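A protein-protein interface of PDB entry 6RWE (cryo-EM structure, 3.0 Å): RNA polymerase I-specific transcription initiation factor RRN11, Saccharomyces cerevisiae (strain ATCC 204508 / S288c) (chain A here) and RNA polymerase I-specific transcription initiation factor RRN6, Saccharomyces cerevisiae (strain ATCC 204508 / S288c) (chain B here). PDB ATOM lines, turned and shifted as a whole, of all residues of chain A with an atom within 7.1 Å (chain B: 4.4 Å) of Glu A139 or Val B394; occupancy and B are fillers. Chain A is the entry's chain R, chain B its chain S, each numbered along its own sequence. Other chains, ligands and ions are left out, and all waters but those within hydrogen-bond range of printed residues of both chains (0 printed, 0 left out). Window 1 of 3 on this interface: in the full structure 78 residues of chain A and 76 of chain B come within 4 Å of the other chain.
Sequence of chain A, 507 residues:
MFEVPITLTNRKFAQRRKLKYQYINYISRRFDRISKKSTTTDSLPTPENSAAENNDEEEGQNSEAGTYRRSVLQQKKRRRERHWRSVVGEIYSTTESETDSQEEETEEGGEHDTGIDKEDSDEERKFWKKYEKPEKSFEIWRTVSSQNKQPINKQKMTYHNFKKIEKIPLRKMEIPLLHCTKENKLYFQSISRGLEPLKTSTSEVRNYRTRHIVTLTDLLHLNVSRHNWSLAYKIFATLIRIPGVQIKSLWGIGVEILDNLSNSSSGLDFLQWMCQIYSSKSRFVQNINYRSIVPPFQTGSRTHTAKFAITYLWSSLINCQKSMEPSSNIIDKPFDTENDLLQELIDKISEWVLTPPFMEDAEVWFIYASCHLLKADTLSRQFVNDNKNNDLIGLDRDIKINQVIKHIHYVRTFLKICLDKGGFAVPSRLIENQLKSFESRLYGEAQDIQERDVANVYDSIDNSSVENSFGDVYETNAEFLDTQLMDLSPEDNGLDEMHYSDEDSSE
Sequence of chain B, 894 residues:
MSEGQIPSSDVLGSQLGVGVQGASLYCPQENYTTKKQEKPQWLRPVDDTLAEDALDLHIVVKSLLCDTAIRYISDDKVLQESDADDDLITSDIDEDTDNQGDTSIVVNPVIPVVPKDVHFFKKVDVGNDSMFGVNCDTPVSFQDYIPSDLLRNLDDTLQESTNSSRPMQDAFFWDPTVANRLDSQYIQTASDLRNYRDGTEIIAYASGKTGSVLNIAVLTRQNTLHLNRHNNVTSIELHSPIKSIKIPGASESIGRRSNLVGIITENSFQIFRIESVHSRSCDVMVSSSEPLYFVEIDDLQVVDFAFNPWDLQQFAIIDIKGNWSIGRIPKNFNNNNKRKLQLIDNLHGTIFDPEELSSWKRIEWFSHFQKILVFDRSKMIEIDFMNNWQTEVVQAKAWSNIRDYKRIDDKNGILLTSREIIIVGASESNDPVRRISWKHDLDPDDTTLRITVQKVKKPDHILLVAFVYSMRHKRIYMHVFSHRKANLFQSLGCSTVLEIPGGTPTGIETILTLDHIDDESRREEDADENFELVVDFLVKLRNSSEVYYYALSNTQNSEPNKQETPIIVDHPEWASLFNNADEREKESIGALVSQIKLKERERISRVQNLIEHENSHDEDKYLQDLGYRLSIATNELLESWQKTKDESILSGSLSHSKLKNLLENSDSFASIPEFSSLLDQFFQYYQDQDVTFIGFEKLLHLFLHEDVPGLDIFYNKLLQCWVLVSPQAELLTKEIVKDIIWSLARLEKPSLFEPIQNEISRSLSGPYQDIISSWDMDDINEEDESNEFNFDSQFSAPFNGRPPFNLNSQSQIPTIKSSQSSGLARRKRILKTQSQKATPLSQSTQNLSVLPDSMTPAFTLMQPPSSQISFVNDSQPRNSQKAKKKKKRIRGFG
O of Met B380 lies within hydrogen-bond range of N of Val B393, at 3.0 Å.
N of Met B380 is in hydrogen-bond range of O of Val B394.
The side-chain hydroxyl of Ser B418 lies close to the side-chain hydroxyl of Ser B400, 3.5 Å away.
Hydrophobic or aromatic side chains of chain A within 4 Å of the printed part of chain B: Phe A138, Ile A140 and Trp A141.
Among the printed residues, 13 pairs touch across the chains.
O of Val B393 lies within hydrogen-bond range of N of Arg A142, at 3.1 Å.
The backbone carbonyl oxygen (O) of Gln B395 sits at hydrogen-bond distance from the backbone NH (N) of Ile A140 (3.2 Å).
OG of Ser B400 lies close to OE2 of Glu A139 (3.5 Å).
The side-chain hydroxyl (OG) of Ser B418 lies within hydrogen-bond range of the side-chain carboxylate (OE2) of Glu A139.
Among the printed residues, pairs that only touch across the chains: Phe A138 with Ser B400, Glu A139 with Val B394, Glu A139 with Gln B395, Glu A139 with Ala B396, Glu A139 with Ile B423, Ile A140 with Val B393, Trp A141 with Val B393, Trp A141 with Val B394 and Trp A141 with Ile B423.
Ser A137 touches none of the printed residues of chain B.
Printed residues of chain B within 4 Å of Glu A139: Val B394, Gln B395, Ala B396, Ser B400, Ser B418 and Ile B423.
Printed residues of chain B within 4 Å of Ile A140: Val B393 and Gln B395.
Of the printed residues of chain B, Arg A142 touches Val B393 (3.1 Å).
Of the printed residues of chain A, Val B393 touches Ile A140 (3.6 Å), Trp A141 (3.5 Å) and Arg A142 (3.1 Å).
Of the printed residues of chain A, Ile B423 touches Glu A139 and Trp A141.
The nearest printed residue of chain B that does not touch Glu A139 is Ile B402 (4.3 Å).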
ATOM      1  N   PRO A 134      19.953 -20.461  27.443  1.00  0.00           N
ATOM      2  CA  PRO A 134      20.895 -21.585  27.480  1.00  0.00           C
ATOM      3  C   PRO A 134      21.250 -22.106  28.860  1.00  0.00           C
ATOM      4  O   PRO A 134      21.308 -23.327  29.039  1.00  0.00           O
ATOM      5  CB  PRO A 134      22.131 -21.013  26.782  1.00  0.00           C
ATOM      6  CG  PRO A 134      21.626 -19.889  25.971  1.00  0.00           C
ATOM      7  CD  PRO A 134      20.531 -19.294  26.767  1.00  0.00           C
ATOM      8  N   GLU A 135      21.619 -21.212  29.787  1.00  0.00           N
ATOM      9  CA  GLU A 135      21.753 -21.469  31.227  1.00  0.00           C
ATOM     10  C   GLU A 135      22.973 -22.334  31.566  1.00  0.00           C
ATOM     11  O   GLU A 135      23.320 -22.495  32.737  1.00  0.00           O
ATOM     12  CB  GLU A 135      20.439 -22.065  31.767  1.00  0.00           C
ATOM     13  CG  GLU A 135      20.183 -21.986  33.257  1.00  0.00           C
ATOM     14  CD  GLU A 135      20.566 -23.234  34.000  1.00  0.00           C
ATOM     15  OE1 GLU A 135      20.596 -24.308  33.368  1.00  0.00           O
ATOM     16  OE2 GLU A 135      20.784 -23.143  35.227  1.00  0.00           O
ATOM     17  N   LYS A 136      23.662 -22.848  30.550  1.00  0.00           N
ATOM     18  CA  LYS A 136      24.961 -23.493  30.663  1.00  0.00           C
ATOM     19  C   LYS A 136      26.042 -22.722  29.940  1.00  0.00           C
ATOM     20  O   LYS A 136      27.219 -22.848  30.278  1.00  0.00           O
ATOM     21  CB  LYS A 136      24.909 -24.906  30.070  1.00  0.00           C
ATOM     22  CG  LYS A 136      23.974 -25.876  30.763  1.00  0.00           C
ATOM     23  CD  LYS A 136      24.536 -26.369  32.071  1.00  0.00           C
ATOM     24  CE  LYS A 136      25.671 -27.342  31.825  1.00  0.00           C
ATOM     25  NZ  LYS A 136      26.174 -27.940  33.094  1.00  0.00           N
ATOM     26  N   SER A 137      25.650 -21.943  28.940  1.00  0.00           N
ATOM     27  CA  SER A 137      26.548 -21.188  28.089  1.00  0.00           C
ATOM     28  C   SER A 137      25.907 -19.852  27.782  1.00  0.00           C
ATOM     29  O   SER A 137      24.744 -19.611  28.107  1.00  0.00           O
ATOM     30  CB  SER A 137      26.848 -21.941  26.794  1.00  0.00           C
ATOM     31  OG  SER A 137      25.662 -22.126  26.052  1.00  0.00           O
ATOM     32  N   PHE A 138      26.679 -18.968  27.161  1.00  0.00           N
ATOM     33  CA  PHE A 138      26.105 -17.704  26.729  1.00  0.00           C
ATOM     34  C   PHE A 138      25.169 -17.921  25.557  1.00  0.00           C
ATOM     35  O   PHE A 138      24.107 -17.297  25.468  1.00  0.00           O
ATOM     36  CB  PHE A 138      27.206 -16.712  26.352  1.00  0.00           C
ATOM     37  CG  PHE A 138      28.085 -16.315  27.504  1.00  0.00           C
ATOM     38  CD1 PHE A 138      27.696 -15.314  28.378  1.00  0.00           C
ATOM     39  CD2 PHE A 138      29.301 -16.945  27.714  1.00  0.00           C
ATOM     40  CE1 PHE A 138      28.503 -14.949  29.439  1.00  0.00           C
ATOM     41  CE2 PHE A 138      30.112 -16.582  28.772  1.00  0.00           C
ATOM     42  CZ  PHE A 138      29.712 -15.584  29.637  1.00  0.00           C
ATOM     43  N   GLU A 139      25.552 -18.809  24.655  1.00  0.00           N
ATOM     44  CA  GLU A 139      24.808 -19.114  23.451  1.00  0.00           C
ATOM     45  C   GLU A 139      24.392 -20.572  23.496  1.00  0.00           C
ATOM     46  O   GLU A 139      25.177 -21.429  23.906  1.00  0.00           O
ATOM     47  CB  GLU A 139      25.681 -18.862  22.235  1.00  0.00           C
ATOM     48  CG  GLU A 139      26.075 -17.428  22.093  1.00  0.00           C
ATOM     49  CD  GLU A 139      27.164 -17.236  21.076  1.00  0.00           C
ATOM     50  OE1 GLU A 139      27.752 -18.249  20.647  1.00  0.00           O
ATOM     51  OE2 GLU A 139      27.434 -16.076  20.701  1.00  0.00           O
ATOM     52  N   ILE A 140      23.166 -20.864  23.080  1.00  0.00           N
ATOM     53  CA  ILE A 140      22.783 -22.265  23.012  1.00  0.00           C
ATOM     54  C   ILE A 140      23.379 -22.862  21.744  1.00  0.00           C
ATOM     55  O   ILE A 140      22.843 -22.723  20.640  1.00  0.00           O
ATOM     56  CB  ILE A 140      21.257 -22.457  23.142  1.00  0.00           C
ATOM     57  CG1 ILE A 140      20.856 -23.914  22.891  1.00  0.00           C
ATOM     58  CG2 ILE A 140      20.466 -21.409  22.386  1.00  0.00           C
ATOM     59  CD1 ILE A 140      19.450 -24.224  23.306  1.00  0.00           C
ATOM     60  N   TRP A 141      24.546 -23.474  21.904  1.00  0.00           N
ATOM     61  CA  TRP A 141      25.221 -24.160  20.820  1.00  0.00           C
ATOM     62  C   TRP A 141      24.542 -25.485  20.531  1.00  0.00           C
ATOM     63  O   TRP A 141      24.121 -26.198  21.445  1.00  0.00           O
ATOM     64  CB  TRP A 141      26.674 -24.420  21.190  1.00  0.00           C
ATOM     65  CG  TRP A 141      27.520 -23.220  21.245  1.00  0.00           C
ATOM     66  CD1 TRP A 141      27.685 -22.396  22.303  1.00  0.00           C
ATOM     67  CD2 TRP A 141      28.402 -22.754  20.231  1.00  0.00           C
ATOM     68  NE1 TRP A 141      28.581 -21.409  21.999  1.00  0.00           N
ATOM     69  CE2 TRP A 141      29.042 -21.613  20.729  1.00  0.00           C
ATOM     70  CE3 TRP A 141      28.696 -23.176  18.939  1.00  0.00           C
ATOM     71  CZ2 TRP A 141      29.959 -20.891  19.985  1.00  0.00           C
ATOM     72  CZ3 TRP A 141      29.619 -22.461  18.203  1.00  0.00           C
ATOM     73  CH2 TRP A 141      30.237 -21.330  18.727  1.00  0.00           C
ATOM     74  N   ARG A 142      24.442 -25.817  19.253  1.00  0.00           N
ATOM     75  CA  ARG A 142      23.938 -27.108  18.822  1.00  0.00           C
ATOM     76  C   ARG A 142      24.970 -27.708  17.892  1.00  0.00           C
ATOM     77  O   ARG A 142      25.421 -27.040  16.958  1.00  0.00           O
ATOM     78  CB  ARG A 142      22.588 -26.980  18.121  1.00  0.00           C
ATOM     79  CG  ARG A 142      21.488 -26.542  19.048  1.00  0.00           C
ATOM     80  CD  ARG A 142      20.155 -26.434  18.349  1.00  0.00           C
ATOM     81  NE  ARG A 142      19.130 -25.953  19.266  1.00  0.00           N
ATOM     82  CZ  ARG A 142      17.866 -25.727  18.930  1.00  0.00           C
ATOM     83  NH1 ARG A 142      17.462 -25.944  17.687  1.00  0.00           N
ATOM     84  NH2 ARG A 142      17.005 -25.288  19.838  1.00  0.00           N
ATOM     85  N   PRO A 296      25.727 -18.205  33.220  1.00  0.00           N
ATOM     86  CA  PRO A 296      26.847 -19.142  32.991  1.00  0.00           C
ATOM     87  C   PRO A 296      28.125 -18.886  33.775  1.00  0.00           C
ATOM     88  O   PRO A 296      29.081 -19.634  33.581  1.00  0.00           O
ATOM     89  CB  PRO A 296      27.124 -18.996  31.493  1.00  0.00           C
ATOM     90  CG  PRO A 296      25.947 -18.405  30.947  1.00  0.00           C
ATOM     91  CD  PRO A 296      25.487 -17.468  31.966  1.00  0.00           C
ATOM     92  N   LYS B 379      22.695 -15.425  15.017  1.00  0.00           N
ATOM     93  CA  LYS B 379      22.974 -16.844  14.828  1.00  0.00           C
ATOM     94  C   LYS B 379      24.067 -17.026  13.786  1.00  0.00           C
ATOM     95  O   LYS B 379      24.430 -16.103  13.057  1.00  0.00           O
ATOM     96  CB  LYS B 379      21.725 -17.640  14.420  1.00  0.00           C
ATOM     97  CG  LYS B 379      21.251 -17.462  12.998  1.00  0.00           C
ATOM     98  CD  LYS B 379      20.306 -16.293  12.867  1.00  0.00           C
ATOM     99  CE  LYS B 379      19.607 -16.292  11.526  1.00  0.00           C
ATOM    100  NZ  LYS B 379      18.760 -15.086  11.362  1.00  0.00           N
ATOM    101  N   MET B 380      24.594 -18.245  13.736  1.00  0.00           N
ATOM    102  CA  MET B 380      25.545 -18.669  12.720  1.00  0.00           C
ATOM    103  C   MET B 380      24.927 -19.820  11.945  1.00  0.00           C
ATOM    104  O   MET B 380      24.593 -20.856  12.528  1.00  0.00           O
ATOM    105  CB  MET B 380      26.874 -19.089  13.338  1.00  0.00           C
ATOM    106  CG  MET B 380      27.872 -19.626  12.343  1.00  0.00           C
ATOM    107  SD  MET B 380      29.467 -19.992  13.095  1.00  0.00           S
ATOM    108  CE  MET B 380      29.065 -21.448  14.035  1.00  0.00           C
ATOM    109  N   GLU B 392      21.738 -24.528  11.854  1.00  0.00           N
ATOM    110  CA  GLU B 392      22.029 -23.456  12.796  1.00  0.00           C
ATOM    111  C   GLU B 392      22.897 -23.998  13.922  1.00  0.00           C
ATOM    112  O   GLU B 392      22.544 -24.995  14.557  1.00  0.00           O
ATOM    113  CB  GLU B 392      20.739 -22.875  13.366  1.00  0.00           C
ATOM    114  CG  GLU B 392      20.981 -21.721  14.310  1.00  0.00           C
ATOM    115  CD  GLU B 392      19.700 -21.101  14.830  1.00  0.00           C
ATOM    116  OE1 GLU B 392      18.610 -21.589  14.470  1.00  0.00           O
ATOM    117  OE2 GLU B 392      19.783 -20.120  15.598  1.00  0.00           O
ATOM    118  N   VAL B 393      24.021 -23.335  14.184  1.00  0.00           N
ATOM    119  CA  VAL B 393      24.926 -23.796  15.228  1.00  0.00           C
ATOM    120  C   VAL B 393      24.861 -22.868  16.433  1.00  0.00           C
ATOM    121  O   VAL B 393      24.474 -23.280  17.531  1.00  0.00           O
ATOM    122  CB  VAL B 393      26.362 -23.900  14.697  1.00  0.00           C
ATOM    123  CG1 VAL B 393      27.291 -24.342  15.802  1.00  0.00           C
ATOM    124  CG2 VAL B 393      26.423 -24.849  13.518  1.00  0.00           C
ATOM    125  N   VAL B 394      25.241 -21.618  16.238  1.00  0.00           N
ATOM    126  CA  VAL B 394      25.104 -20.595  17.264  1.00  0.00           C
ATOM    127  C   VAL B 394      23.655 -20.143  17.313  1.00  0.00           C
ATOM    128  O   VAL B 394      23.014 -19.966  16.275  1.00  0.00           O
ATOM    129  CB  VAL B 394      26.046 -19.418  16.959  1.00  0.00           C
ATOM    130  CG1 VAL B 394      25.857 -18.285  17.930  1.00  0.00           C
ATOM    131  CG2 VAL B 394      27.473 -19.869  16.990  1.00  0.00           C
ATOM    132  N   GLN B 395      23.114 -19.986  18.514  1.00  0.00           N
ATOM    133  CA  GLN B 395      21.891 -19.218  18.700  1.00  0.00           C
ATOM    134  C   GLN B 395      22.158 -18.220  19.816  1.00  0.00           C
ATOM    135  O   GLN B 395      22.352 -18.603  20.972  1.00  0.00           O
ATOM    136  CB  GLN B 395      20.707 -20.119  19.011  1.00  0.00           C
ATOM    137  CG  GLN B 395      19.391 -19.404  19.065  1.00  0.00           C
ATOM    138  CD  GLN B 395      18.262 -20.363  19.310  1.00  0.00           C
ATOM    139  OE1 GLN B 395      18.483 -21.552  19.526  1.00  0.00           O
ATOM    140  NE2 GLN B 395      17.044 -19.868  19.253  1.00  0.00           N
ATOM    141  N   ALA B 396      22.168 -16.940  19.460  1.00  0.00           N
ATOM    142  CA  ALA B 396      22.785 -15.888  20.254  1.00  0.00           C
ATOM    143  C   ALA B 396      21.775 -14.775  20.505  1.00  0.00           C
ATOM    144  O   ALA B 396      21.956 -13.638  20.080  1.00  0.00           O
ATOM    145  CB  ALA B 396      24.035 -15.351  19.570  1.00  0.00           C
ATOM    146  N   SER B 400      23.853 -12.907  24.783  1.00  0.00           N
ATOM    147  CA  SER B 400      24.962 -12.358  24.029  1.00  0.00           C
ATOM    148  C   SER B 400      24.522 -12.170  22.591  1.00  0.00           C
ATOM    149  O   SER B 400      23.433 -12.573  22.198  1.00  0.00           O
ATOM    150  CB  SER B 400      26.201 -13.248  24.109  1.00  0.00           C
ATOM    151  OG  SER B 400      25.976 -14.464  23.438  1.00  0.00           O
ATOM    152  N   ILE B 402      26.498 -11.582  18.410  1.00  0.00           N
ATOM    153  CA  ILE B 402      27.710 -11.838  17.652  1.00  0.00           C
ATOM    154  C   ILE B 402      28.240 -10.508  17.147  1.00  0.00           C
ATOM    155  O   ILE B 402      27.496  -9.721  16.557  1.00  0.00           O
ATOM    156  CB  ILE B 402      27.429 -12.798  16.492  1.00  0.00           C
ATOM    157  CG1 ILE B 402      26.729 -14.045  17.019  1.00  0.00           C
ATOM    158  CG2 ILE B 402      28.724 -13.200  15.837  1.00  0.00           C
ATOM    159  CD1 ILE B 402      26.105 -14.881  15.939  1.00  0.00           C
ATOM    160  N   SER B 418      31.977 -13.014  19.954  1.00  0.00           N
ATOM    161  CA  SER B 418      30.703 -12.559  20.464  1.00  0.00           C
ATOM    162  C   SER B 418      30.955 -11.407  21.421  1.00  0.00           C
ATOM    163  O   SER B 418      32.095 -11.066  21.734  1.00  0.00           O
ATOM    164  CB  SER B 418      29.967 -13.696  21.161  1.00  0.00           C
ATOM    165  OG  SER B 418      28.781 -13.226  21.767  1.00  0.00           O
ATOM    166  N   ILE B 423      35.654 -16.723  21.081  1.00  0.00           N
ATOM    167  CA  ILE B 423      35.497 -18.142  20.782  1.00  0.00           C
ATOM    168  C   ILE B 423      36.417 -18.508  19.626  1.00  0.00           C
ATOM    169  O   ILE B 423      36.425 -17.825  18.598  1.00  0.00           O
ATOM    170  CB  ILE B 423      34.035 -18.474  20.447  1.00  0.00           C
ATOM    171  CG1 ILE B 423      33.131 -18.042  21.592  1.00  0.00           C
ATOM    172  CG2 ILE B 423      33.863 -19.953  20.230  1.00  0.00           C
ATOM    173  CD1 ILE B 423      31.687 -18.019  21.234  1.00  0.00           C
